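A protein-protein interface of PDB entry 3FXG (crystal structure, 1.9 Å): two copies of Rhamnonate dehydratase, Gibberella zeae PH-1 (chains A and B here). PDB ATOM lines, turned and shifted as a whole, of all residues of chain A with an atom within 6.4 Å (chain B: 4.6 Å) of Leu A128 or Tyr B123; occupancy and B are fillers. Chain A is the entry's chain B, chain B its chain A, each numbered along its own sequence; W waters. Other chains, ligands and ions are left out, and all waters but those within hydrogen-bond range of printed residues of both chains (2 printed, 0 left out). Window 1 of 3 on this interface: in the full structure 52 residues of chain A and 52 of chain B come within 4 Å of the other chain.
The side-chain hydroxyl of Tyr A278 sits at hydrogen-bond distance from the backbone carbonyl oxygen of Phe B122. N of Leu A128 lies within hydrogen-bond range of O of Tyr B123, 3.0 Å away.
The side-chain hydroxyl of Tyr B123 is in hydrogen-bond range of a ring nitrogen (ND1) of His B96 (2.7 Å). The side-chain sulfur (SD) of Met A225 sits at hydrogen-bond distance from a ring nitrogen (ND1) of His A276.
Among the printed residues, merely in contact across the chains: Gly A127 with Tyr B123 (3.3 Å), Gly A60 with Phe B122 (3.3 Å), His A276 with Phe B122 (3.5 Å), Met A225 with Met B121 (3.7 Å), Val A63 with His B96 (3.8 Å), Met A225 with Phe B122 (3.8 Å), Leu A64 with Tyr B123 (3.9 Å), Phe A84 with Phe B122 (3.9 Å) and Phe A84 with Tyr B123 (3.9 Å).
Of chain B, only Tyr B123 (3.0 Å) comes within 4 Å of Leu A128. Of the printed residues of chain B, Met A225 touches Met B121 (3.7 Å) and Phe B122 (3.8 Å). Of the printed residues of chain B, Tyr A278 touches Phe B122 (3.5 Å). Of the printed residues of chain A, Met B121 touches Met A225 (3.7 Å). Tyr B123 touches just these residues of chain A: Leu A64, Phe A84, Gly A127 and Leu A128. The nearest printed residue of chain B that does not touch Leu A128 is Pro B129 (4.6 Å). The nearest printed residue of chain B that does not touch Tyr A278 is Tyr B123 (4.2 Å).
Printed residues of chain B that touch a printed residue of chain A: His B96, Met B121, Phe B122 and Tyr B123. Hydrophobic or aromatic side chains of chain B that line the printed part of chain A: His B96, Met B121, Phe B122 and Tyr B123. Printed residues of chain A that touch a printed residue of chain B: Gly A60, Val A63, Leu A64, Phe A84, Gly A127, Leu A128, Met A225, His A276 and Tyr A278. Hydrophobic or aromatic side chains of chain A within 4 Å of the printed part of chain B: Val A63, Leu A64, Phe A84, Met A225, His A276 and Tyr A278. Among the printed residues, 11 pairs touch across the chains.
Positions printed for both chains: 92 and 129. Of the 11 pairs that touch across the chains among the printed residues, none has its exchanged pair printed and touching as well.
Water W2 lies within hydrogen-bond range of the backbone carbonyl oxygen of Met B121, the side-chain hydroxyl of Tyr A278 and the backbone carbonyl oxygen of His A276. Water W1 lies within hydrogen-bond range of the side-chain hydroxyl of Tyr A278 and the backbone carbonyl oxygen of Phe B122.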
ATOM      1  N   GLY A  60      -2.635  13.345 -14.355  1.00  0.00           N
ATOM      2  CA  GLY A  60      -2.118  13.679 -13.036  1.00  0.00           C
ATOM      3  C   GLY A  60      -2.218  15.078 -12.454  1.00  0.00           C
ATOM      4  O   GLY A  60      -1.350  15.468 -11.671  1.00  0.00           O
ATOM      5  N   VAL A  63      -2.185  14.716  -8.783  1.00  0.00           N
ATOM      6  CA  VAL A  63      -1.139  13.869  -8.219  1.00  0.00           C
ATOM      7  C   VAL A  63      -0.528  14.288  -6.878  1.00  0.00           C
ATOM      8  O   VAL A  63      -0.264  13.439  -6.029  1.00  0.00           O
ATOM      9  CB  VAL A  63       0.006  13.653  -9.252  1.00  0.00           C
ATOM     10  CG1 VAL A  63       0.884  14.895  -9.341  1.00  0.00           C
ATOM     11  CG2 VAL A  63       0.822  12.431  -8.872  1.00  0.00           C
ATOM     12  N   LEU A  64      -0.312  15.581  -6.669  1.00  0.00           N
ATOM     13  CA  LEU A  64       0.309  16.039  -5.426  1.00  0.00           C
ATOM     14  C   LEU A  64      -0.556  15.986  -4.167  1.00  0.00           C
ATOM     15  O   LEU A  64      -0.110  15.505  -3.124  1.00  0.00           O
ATOM     16  CB  LEU A  64       0.853  17.459  -5.604  1.00  0.00           C
ATOM     17  CG  LEU A  64       1.929  17.646  -6.679  1.00  0.00           C
ATOM     18  CD1 LEU A  64       2.394  19.097  -6.674  1.00  0.00           C
ATOM     19  CD2 LEU A  64       3.099  16.714  -6.412  1.00  0.00           C
ATOM     20  N   PHE A  84      -1.038  23.079  -2.197  1.00  0.00           N
ATOM     21  CA  PHE A  84      -0.883  21.789  -2.844  1.00  0.00           C
ATOM     22  C   PHE A  84       0.591  21.427  -2.751  1.00  0.00           C
ATOM     23  O   PHE A  84       1.440  22.303  -2.596  1.00  0.00           O
ATOM     24  CB  PHE A  84      -1.374  21.823  -4.306  1.00  0.00           C
ATOM     25  CG  PHE A  84      -0.352  22.307  -5.309  1.00  0.00           C
ATOM     26  CD1 PHE A  84      -0.276  21.712  -6.567  1.00  0.00           C
ATOM     27  CD2 PHE A  84       0.511  23.360  -5.018  1.00  0.00           C
ATOM     28  CE1 PHE A  84       0.646  22.157  -7.521  1.00  0.00           C
ATOM     29  CE2 PHE A  84       1.437  23.810  -5.966  1.00  0.00           C
ATOM     30  CZ  PHE A  84       1.502  23.208  -7.217  1.00  0.00           C
ATOM     31  N   GLY A  85       0.891  20.137  -2.823  1.00  0.00           N
ATOM     32  CA  GLY A  85       2.268  19.699  -2.722  1.00  0.00           C
ATOM     33  C   GLY A  85       2.322  18.345  -2.047  1.00  0.00           C
ATOM     34  O   GLY A  85       3.240  17.564  -2.280  1.00  0.00           O
ATOM     35  N   GLY A  86       1.335  18.076  -1.196  1.00  0.00           N
ATOM     36  CA  GLY A  86       1.255  16.796  -0.513  1.00  0.00           C
ATOM     37  C   GLY A  86       2.522  16.274   0.141  1.00  0.00           C
ATOM     38  O   GLY A  86       3.281  17.043   0.732  1.00  0.00           O
ATOM     39  N   PRO A  88       5.593  15.150  -1.010  1.00  0.00           N
ATOM     40  CA  PRO A  88       6.880  15.733  -1.417  1.00  0.00           C
ATOM     41  C   PRO A  88       7.116  17.077  -0.736  1.00  0.00           C
ATOM     42  O   PRO A  88       8.236  17.399  -0.336  1.00  0.00           O
ATOM     43  CB  PRO A  88       6.736  15.900  -2.930  1.00  0.00           C
ATOM     44  CG  PRO A  88       5.687  14.927  -3.309  1.00  0.00           C
ATOM     45  CD  PRO A  88       4.706  14.988  -2.173  1.00  0.00           C
ATOM     46  N   ALA A  89       6.050  17.864  -0.628  1.00  0.00           N
ATOM     47  CA  ALA A  89       6.121  19.177   0.004  1.00  0.00           C
ATOM     48  C   ALA A  89       6.464  19.050   1.486  1.00  0.00           C
ATOM     49  O   ALA A  89       7.318  19.779   1.995  1.00  0.00           O
ATOM     50  CB  ALA A  89       4.798  19.907  -0.164  1.00  0.00           C
ATOM     51  N   LEU A  92      10.140  18.212   2.057  1.00  0.00           N
ATOM     52  CA  LEU A  92      11.017  19.373   1.934  1.00  0.00           C
ATOM     53  C   LEU A  92      10.891  20.321   3.116  1.00  0.00           C
ATOM     54  O   LEU A  92      11.878  20.913   3.554  1.00  0.00           O
ATOM     55  CB  LEU A  92      10.711  20.130   0.638  1.00  0.00           C
ATOM     56  CG  LEU A  92      11.150  19.418  -0.640  1.00  0.00           C
ATOM     57  CD1 LEU A  92      10.615  20.163  -1.851  1.00  0.00           C
ATOM     58  CD2 LEU A  92      12.673  19.337  -0.680  1.00  0.00           C
ATOM     59  N   LYS A 126      11.442  27.784  -9.285  1.00  0.00           N
ATOM     60  CA  LYS A 126      10.076  27.676  -9.769  1.00  0.00           C
ATOM     61  C   LYS A 126       9.504  26.319  -9.378  1.00  0.00           C
ATOM     62  O   LYS A 126      10.236  25.432  -8.931  1.00  0.00           O
ATOM     63  CB  LYS A 126      10.031  27.856 -11.295  1.00  0.00           C
ATOM     64  CG  LYS A 126      10.538  29.223 -11.761  1.00  0.00           C
ATOM     65  CD  LYS A 126      10.377  29.424 -13.254  1.00  0.00           C
ATOM     66  CE  LYS A 126      11.133  30.666 -13.720  1.00  0.00           C
ATOM     67  NZ  LYS A 126      10.688  31.911 -13.031  1.00  0.00           N
ATOM     68  N   GLY A 127       8.191  26.180  -9.513  1.00  0.00           N
ATOM     69  CA  GLY A 127       7.543  24.918  -9.209  1.00  0.00           C
ATOM     70  C   GLY A 127       7.317  24.533  -7.759  1.00  0.00           C
ATOM     71  O   GLY A 127       7.200  25.378  -6.868  1.00  0.00           O
ATOM     72  N   LEU A 128       7.267  23.223  -7.542  1.00  0.00           N
ATOM     73  CA  LEU A 128       7.016  22.620  -6.236  1.00  0.00           C
ATOM     74  C   LEU A 128       7.759  23.207  -5.041  1.00  0.00           C
ATOM     75  O   LEU A 128       7.142  23.519  -4.023  1.00  0.00           O
ATOM     76  CB  LEU A 128       7.278  21.109  -6.313  1.00  0.00           C
ATOM     77  CG  LEU A 128       7.046  20.268  -5.051  1.00  0.00           C
ATOM     78  CD1 LEU A 128       5.618  20.448  -4.541  1.00  0.00           C
ATOM     79  CD2 LEU A 128       7.319  18.806  -5.377  1.00  0.00           C
ATOM     80  N   PRO A 129       9.089  23.362  -5.136  1.00  0.00           N
ATOM     81  CA  PRO A 129       9.820  23.917  -3.994  1.00  0.00           C
ATOM     82  C   PRO A 129       9.307  25.298  -3.590  1.00  0.00           C
ATOM     83  O   PRO A 129       9.238  25.627  -2.405  1.00  0.00           O
ATOM     84  CB  PRO A 129      11.265  23.964  -4.493  1.00  0.00           C
ATOM     85  CG  PRO A 129      11.308  22.880  -5.541  1.00  0.00           C
ATOM     86  CD  PRO A 129      10.005  23.093  -6.257  1.00  0.00           C
ATOM     87  N   ILE A 130       8.942  26.105  -4.579  1.00  0.00           N
ATOM     88  CA  ILE A 130       8.442  27.440  -4.294  1.00  0.00           C
ATOM     89  C   ILE A 130       7.056  27.367  -3.654  1.00  0.00           C
ATOM     90  O   ILE A 130       6.695  28.222  -2.845  1.00  0.00           O
ATOM     91  CB  ILE A 130       8.409  28.298  -5.576  1.00  0.00           C
ATOM     92  CG1 ILE A 130       9.788  28.259  -6.243  1.00  0.00           C
ATOM     93  CG2 ILE A 130       8.035  29.738  -5.242  1.00  0.00           C
ATOM     94  CD1 ILE A 130      10.939  28.600  -5.297  1.00  0.00           C
ATOM     95  N   ALA A 131       6.289  26.340  -4.006  1.00  0.00           N
ATOM     96  CA  ALA A 131       4.958  26.158  -3.431  1.00  0.00           C
ATOM     97  C   ALA A 131       5.124  25.873  -1.935  1.00  0.00           C
ATOM     98  O   ALA A 131       4.323  26.320  -1.113  1.00  0.00           O
ATOM     99  CB  ALA A 131       4.237  24.993  -4.116  1.00  0.00           C
ATOM    100  N   VAL A 132       6.177  25.135  -1.588  1.00  0.00           N
ATOM    101  CA  VAL A 132       6.454  24.805  -0.191  1.00  0.00           C
ATOM    102  C   VAL A 132       6.781  26.075   0.596  1.00  0.00           C
ATOM    103  O   VAL A 132       6.224  26.313   1.669  1.00  0.00           O
ATOM    104  CB  VAL A 132       7.637  23.815  -0.072  1.00  0.00           C
ATOM    105  CG1 VAL A 132       7.924  23.514   1.400  1.00  0.00           C
ATOM    106  CG2 VAL A 132       7.315  22.529  -0.821  1.00  0.00           C
ATOM    107  N   ILE A 133       7.690  26.883   0.057  1.00  0.00           N
ATOM    108  CA  ILE A 133       8.078  28.139   0.693  1.00  0.00           C
ATOM    109  C   ILE A 133       6.841  29.025   0.858  1.00  0.00           C
ATOM    110  O   ILE A 133       6.675  29.694   1.875  1.00  0.00           O
ATOM    111  CB  ILE A 133       9.133  28.893  -0.165  1.00  0.00           C
ATOM    112  CG1 ILE A 133      10.442  28.099  -0.202  1.00  0.00           C
ATOM    113  CG2 ILE A 133       9.391  30.283   0.410  1.00  0.00           C
ATOM    114  CD1 ILE A 133      11.492  28.677  -1.155  1.00  0.00           C
ATOM    115  N   MET A 225      -2.933  27.321 -20.160  1.00  0.00           N
ATOM    116  CA  MET A 225      -1.640  27.192 -20.845  1.00  0.00           C
ATOM    117  C   MET A 225      -1.597  26.143 -21.963  1.00  0.00           C
ATOM    118  O   MET A 225      -0.549  25.556 -22.228  1.00  0.00           O
ATOM    119  CB  MET A 225      -0.532  26.903 -19.808  1.00  0.00           C
ATOM    120  CG  MET A 225      -0.681  25.595 -19.028  1.00  0.00           C
ATOM    121  SD  MET A 225       0.540  25.369 -17.488  1.00  0.00           S
ATOM    122  CE  MET A 225      -0.542  24.122 -16.473  1.00  0.00           C
ATOM    123  N   HIS A 276       1.003  30.175 -13.200  1.00  0.00           N
ATOM    124  CA  HIS A 276       2.063  29.177 -13.179  1.00  0.00           C
ATOM    125  C   HIS A 276       3.453  29.800 -13.325  1.00  0.00           C
ATOM    126  O   HIS A 276       4.371  29.182 -13.867  1.00  0.00           O
ATOM    127  CB  HIS A 276       1.830  28.110 -14.259  1.00  0.00           C
ATOM    128  CG  HIS A 276       0.607  27.276 -14.019  1.00  0.00           C
ATOM    129  ND1 HIS A 276      -0.597  27.521 -14.644  1.00  0.00           N
ATOM    130  CD2 HIS A 276       0.391  26.232 -13.184  1.00  0.00           C
ATOM    131  CE1 HIS A 276      -1.503  26.664 -14.204  1.00  0.00           C
ATOM    132  NE2 HIS A 276      -0.929  25.872 -13.316  1.00  0.00           N
ATOM    133  N   TYR A 278       6.566  32.072 -11.120  1.00  0.00           N
ATOM    134  CA  TYR A 278       7.044  32.172  -9.738  1.00  0.00           C
ATOM    135  C   TYR A 278       8.118  33.228  -9.487  1.00  0.00           C
ATOM    136  O   TYR A 278       8.900  33.560 -10.381  1.00  0.00           O
ATOM    137  CB  TYR A 278       7.609  30.811  -9.306  1.00  0.00           C
ATOM    138  CG  TYR A 278       6.770  29.628  -9.734  1.00  0.00           C
ATOM    139  CD1 TYR A 278       5.918  28.985  -8.836  1.00  0.00           C
ATOM    140  CD2 TYR A 278       6.795  29.178 -11.055  1.00  0.00           C
ATOM    141  CE1 TYR A 278       5.107  27.924  -9.251  1.00  0.00           C
ATOM    142  CE2 TYR A 278       5.992  28.128 -11.474  1.00  0.00           C
ATOM    143  CZ  TYR A 278       5.151  27.509 -10.573  1.00  0.00           C
ATOM    144  OH  TYR A 278       4.339  26.487 -11.011  1.00  0.00           O
ATOM    145  N   LEU B  92       7.704  11.077  -6.863  1.00  0.00           N
ATOM    146  CA  LEU B  92       7.166  11.569  -8.129  1.00  0.00           C
ATOM    147  C   LEU B  92       7.244  10.524  -9.238  1.00  0.00           C
ATOM    148  O   LEU B  92       6.311  10.380 -10.030  1.00  0.00           O
ATOM    149  CB  LEU B  92       7.907  12.840  -8.554  1.00  0.00           C
ATOM    150  CG  LEU B  92       7.672  14.064  -7.664  1.00  0.00           C
ATOM    151  CD1 LEU B  92       8.633  15.178  -8.052  1.00  0.00           C
ATOM    152  CD2 LEU B  92       6.227  14.530  -7.803  1.00  0.00           C
ATOM    153  N   HIS B  96       3.483  10.054 -10.300  1.00  0.00           N
ATOM    154  CA  HIS B  96       3.126  10.783 -11.508  1.00  0.00           C
ATOM    155  C   HIS B  96       3.584  10.198 -12.841  1.00  0.00           C
ATOM    156  O   HIS B  96       2.770   9.926 -13.723  1.00  0.00           O
ATOM    157  CB  HIS B  96       3.631  12.230 -11.406  1.00  0.00           C
ATOM    158  CG  HIS B  96       2.990  13.166 -12.385  1.00  0.00           C
ATOM    159  ND1 HIS B  96       3.368  14.486 -12.509  1.00  0.00           N
ATOM    160  CD2 HIS B  96       1.983  12.980 -13.271  1.00  0.00           C
ATOM    161  CE1 HIS B  96       2.621  15.072 -13.428  1.00  0.00           C
ATOM    162  NE2 HIS B  96       1.773  14.181 -13.906  1.00  0.00           N
ATOM    163  N   PHE B  97       4.885   9.982 -12.985  1.00  0.00           N
ATOM    164  CA  PHE B  97       5.426   9.522 -14.256  1.00  0.00           C
ATOM    165  C   PHE B  97       5.265   8.066 -14.679  1.00  0.00           C
ATOM    166  O   PHE B  97       5.237   7.780 -15.876  1.00  0.00           O
ATOM    167  CB  PHE B  97       6.895   9.950 -14.334  1.00  0.00           C
ATOM    168  CG  PHE B  97       7.092  11.420 -14.095  1.00  0.00           C
ATOM    169  CD1 PHE B  97       6.466  12.357 -14.917  1.00  0.00           C
ATOM    170  CD2 PHE B  97       7.851  11.873 -13.020  1.00  0.00           C
ATOM    171  CE1 PHE B  97       6.590  13.724 -14.666  1.00  0.00           C
ATOM    172  CE2 PHE B  97       7.981  13.237 -12.760  1.00  0.00           C
ATOM    173  CZ  PHE B  97       7.347  14.165 -13.584  1.00  0.00           C
ATOM    174  N   SER B 120       3.536  17.729 -16.179  1.00  0.00           N
ATOM    175  CA  SER B 120       4.010  18.220 -14.888  1.00  0.00           C
ATOM    176  C   SER B 120       4.288  19.720 -14.892  1.00  0.00           C
ATOM    177  O   SER B 120       4.845  20.256 -13.934  1.00  0.00           O
ATOM    178  CB  SER B 120       5.278  17.471 -14.464  1.00  0.00           C
ATOM    179  OG  SER B 120       6.320  17.644 -15.409  1.00  0.00           O
ATOM    180  N   MET B 121       3.903  20.402 -15.967  1.00  0.00           N
ATOM    181  CA  MET B 121       4.141  21.836 -16.047  1.00  0.00           C
ATOM    182  C   MET B 121       3.458  22.630 -14.944  1.00  0.00           C
ATOM    183  O   MET B 121       3.964  23.674 -14.536  1.00  0.00           O
ATOM    184  CB  MET B 121       3.692  22.398 -17.397  1.00  0.00           C
ATOM    185  CG  MET B 121       4.590  22.045 -18.561  1.00  0.00           C
ATOM    186  SD  MET B 121       4.502  23.401 -19.944  1.00  0.00           S
ATOM    187  CE  MET B 121       2.586  23.643 -20.015  1.00  0.00           C
ATOM    188  N   PHE B 122       2.320  22.147 -14.453  1.00  0.00           N
ATOM    189  CA  PHE B 122       1.609  22.887 -13.420  1.00  0.00           C
ATOM    190  C   PHE B 122       2.391  23.000 -12.115  1.00  0.00           C
ATOM    191  O   PHE B 122       2.074  23.836 -11.273  1.00  0.00           O
ATOM    192  CB  PHE B 122       0.203  22.301 -13.187  1.00  0.00           C
ATOM    193  CG  PHE B 122       0.185  20.959 -12.511  1.00  0.00           C
ATOM    194  CD1 PHE B 122      -0.118  20.855 -11.155  1.00  0.00           C
ATOM    195  CD2 PHE B 122       0.425  19.794 -13.236  1.00  0.00           C
ATOM    196  CE1 PHE B 122      -0.187  19.609 -10.531  1.00  0.00           C
ATOM    197  CE2 PHE B 122       0.359  18.542 -12.623  1.00  0.00           C
ATOM    198  CZ  PHE B 122       0.051  18.448 -11.270  1.00  0.00           C
ATOM    199  N   TYR B 123       3.429  22.185 -11.955  1.00  0.00           N
ATOM    200  CA  TYR B 123       4.250  22.263 -10.746  1.00  0.00           C
ATOM    201  C   TYR B 123       5.727  22.089 -11.079  1.00  0.00           C
ATOM    202  O   TYR B 123       6.561  21.968 -10.183  1.00  0.00           O
ATOM    203  CB  TYR B 123       3.807  21.207  -9.721  1.00  0.00           C
ATOM    204  CG  TYR B 123       4.162  19.771 -10.063  1.00  0.00           C
ATOM    205  CD1 TYR B 123       5.370  19.208  -9.644  1.00  0.00           C
ATOM    206  CD2 TYR B 123       3.287  18.976 -10.800  1.00  0.00           C
ATOM    207  CE1 TYR B 123       5.694  17.884  -9.954  1.00  0.00           C
ATOM    208  CE2 TYR B 123       3.600  17.652 -11.116  1.00  0.00           C
ATOM    209  CZ  TYR B 123       4.804  17.114 -10.692  1.00  0.00           C
ATOM    210  OH  TYR B 123       5.122  15.813 -11.018  1.00  0.00           O
ATOM    211  N   GLY B 124       6.054  22.111 -12.368  1.00  0.00           N
ATOM    212  CA  GLY B 124       7.435  21.913 -12.766  1.00  0.00           C
ATOM    213  C   GLY B 124       8.090  22.968 -13.632  1.00  0.00           C
ATOM    214  O   GLY B 124       8.294  24.103 -13.195  1.00  0.00           O
ATOM    215  N   PRO B 129      11.302  18.505 -10.289  1.00  0.00           N
ATOM    216  CA  PRO B 129      10.479  17.666 -11.170  1.00  0.00           C
ATOM    217  C   PRO B 129      11.194  17.316 -12.472  1.00  0.00           C
ATOM    218  O   PRO B 129      11.074  16.198 -12.985  1.00  0.00           O
ATOM    219  CB  PRO B 129       9.241  18.532 -11.413  1.00  0.00           C
ATOM    220  CG  PRO B 129       9.154  19.355 -10.166  1.00  0.00           C
ATOM    221  CD  PRO B 129      10.592  19.742  -9.931  1.00  0.00           C
HETATM  222  O   HOH W   1       2.378  25.813  -9.255  1.00  0.00           O
HETATM  223  O   HOH W   2       4.997  25.861 -13.604  1.00  0.00           O
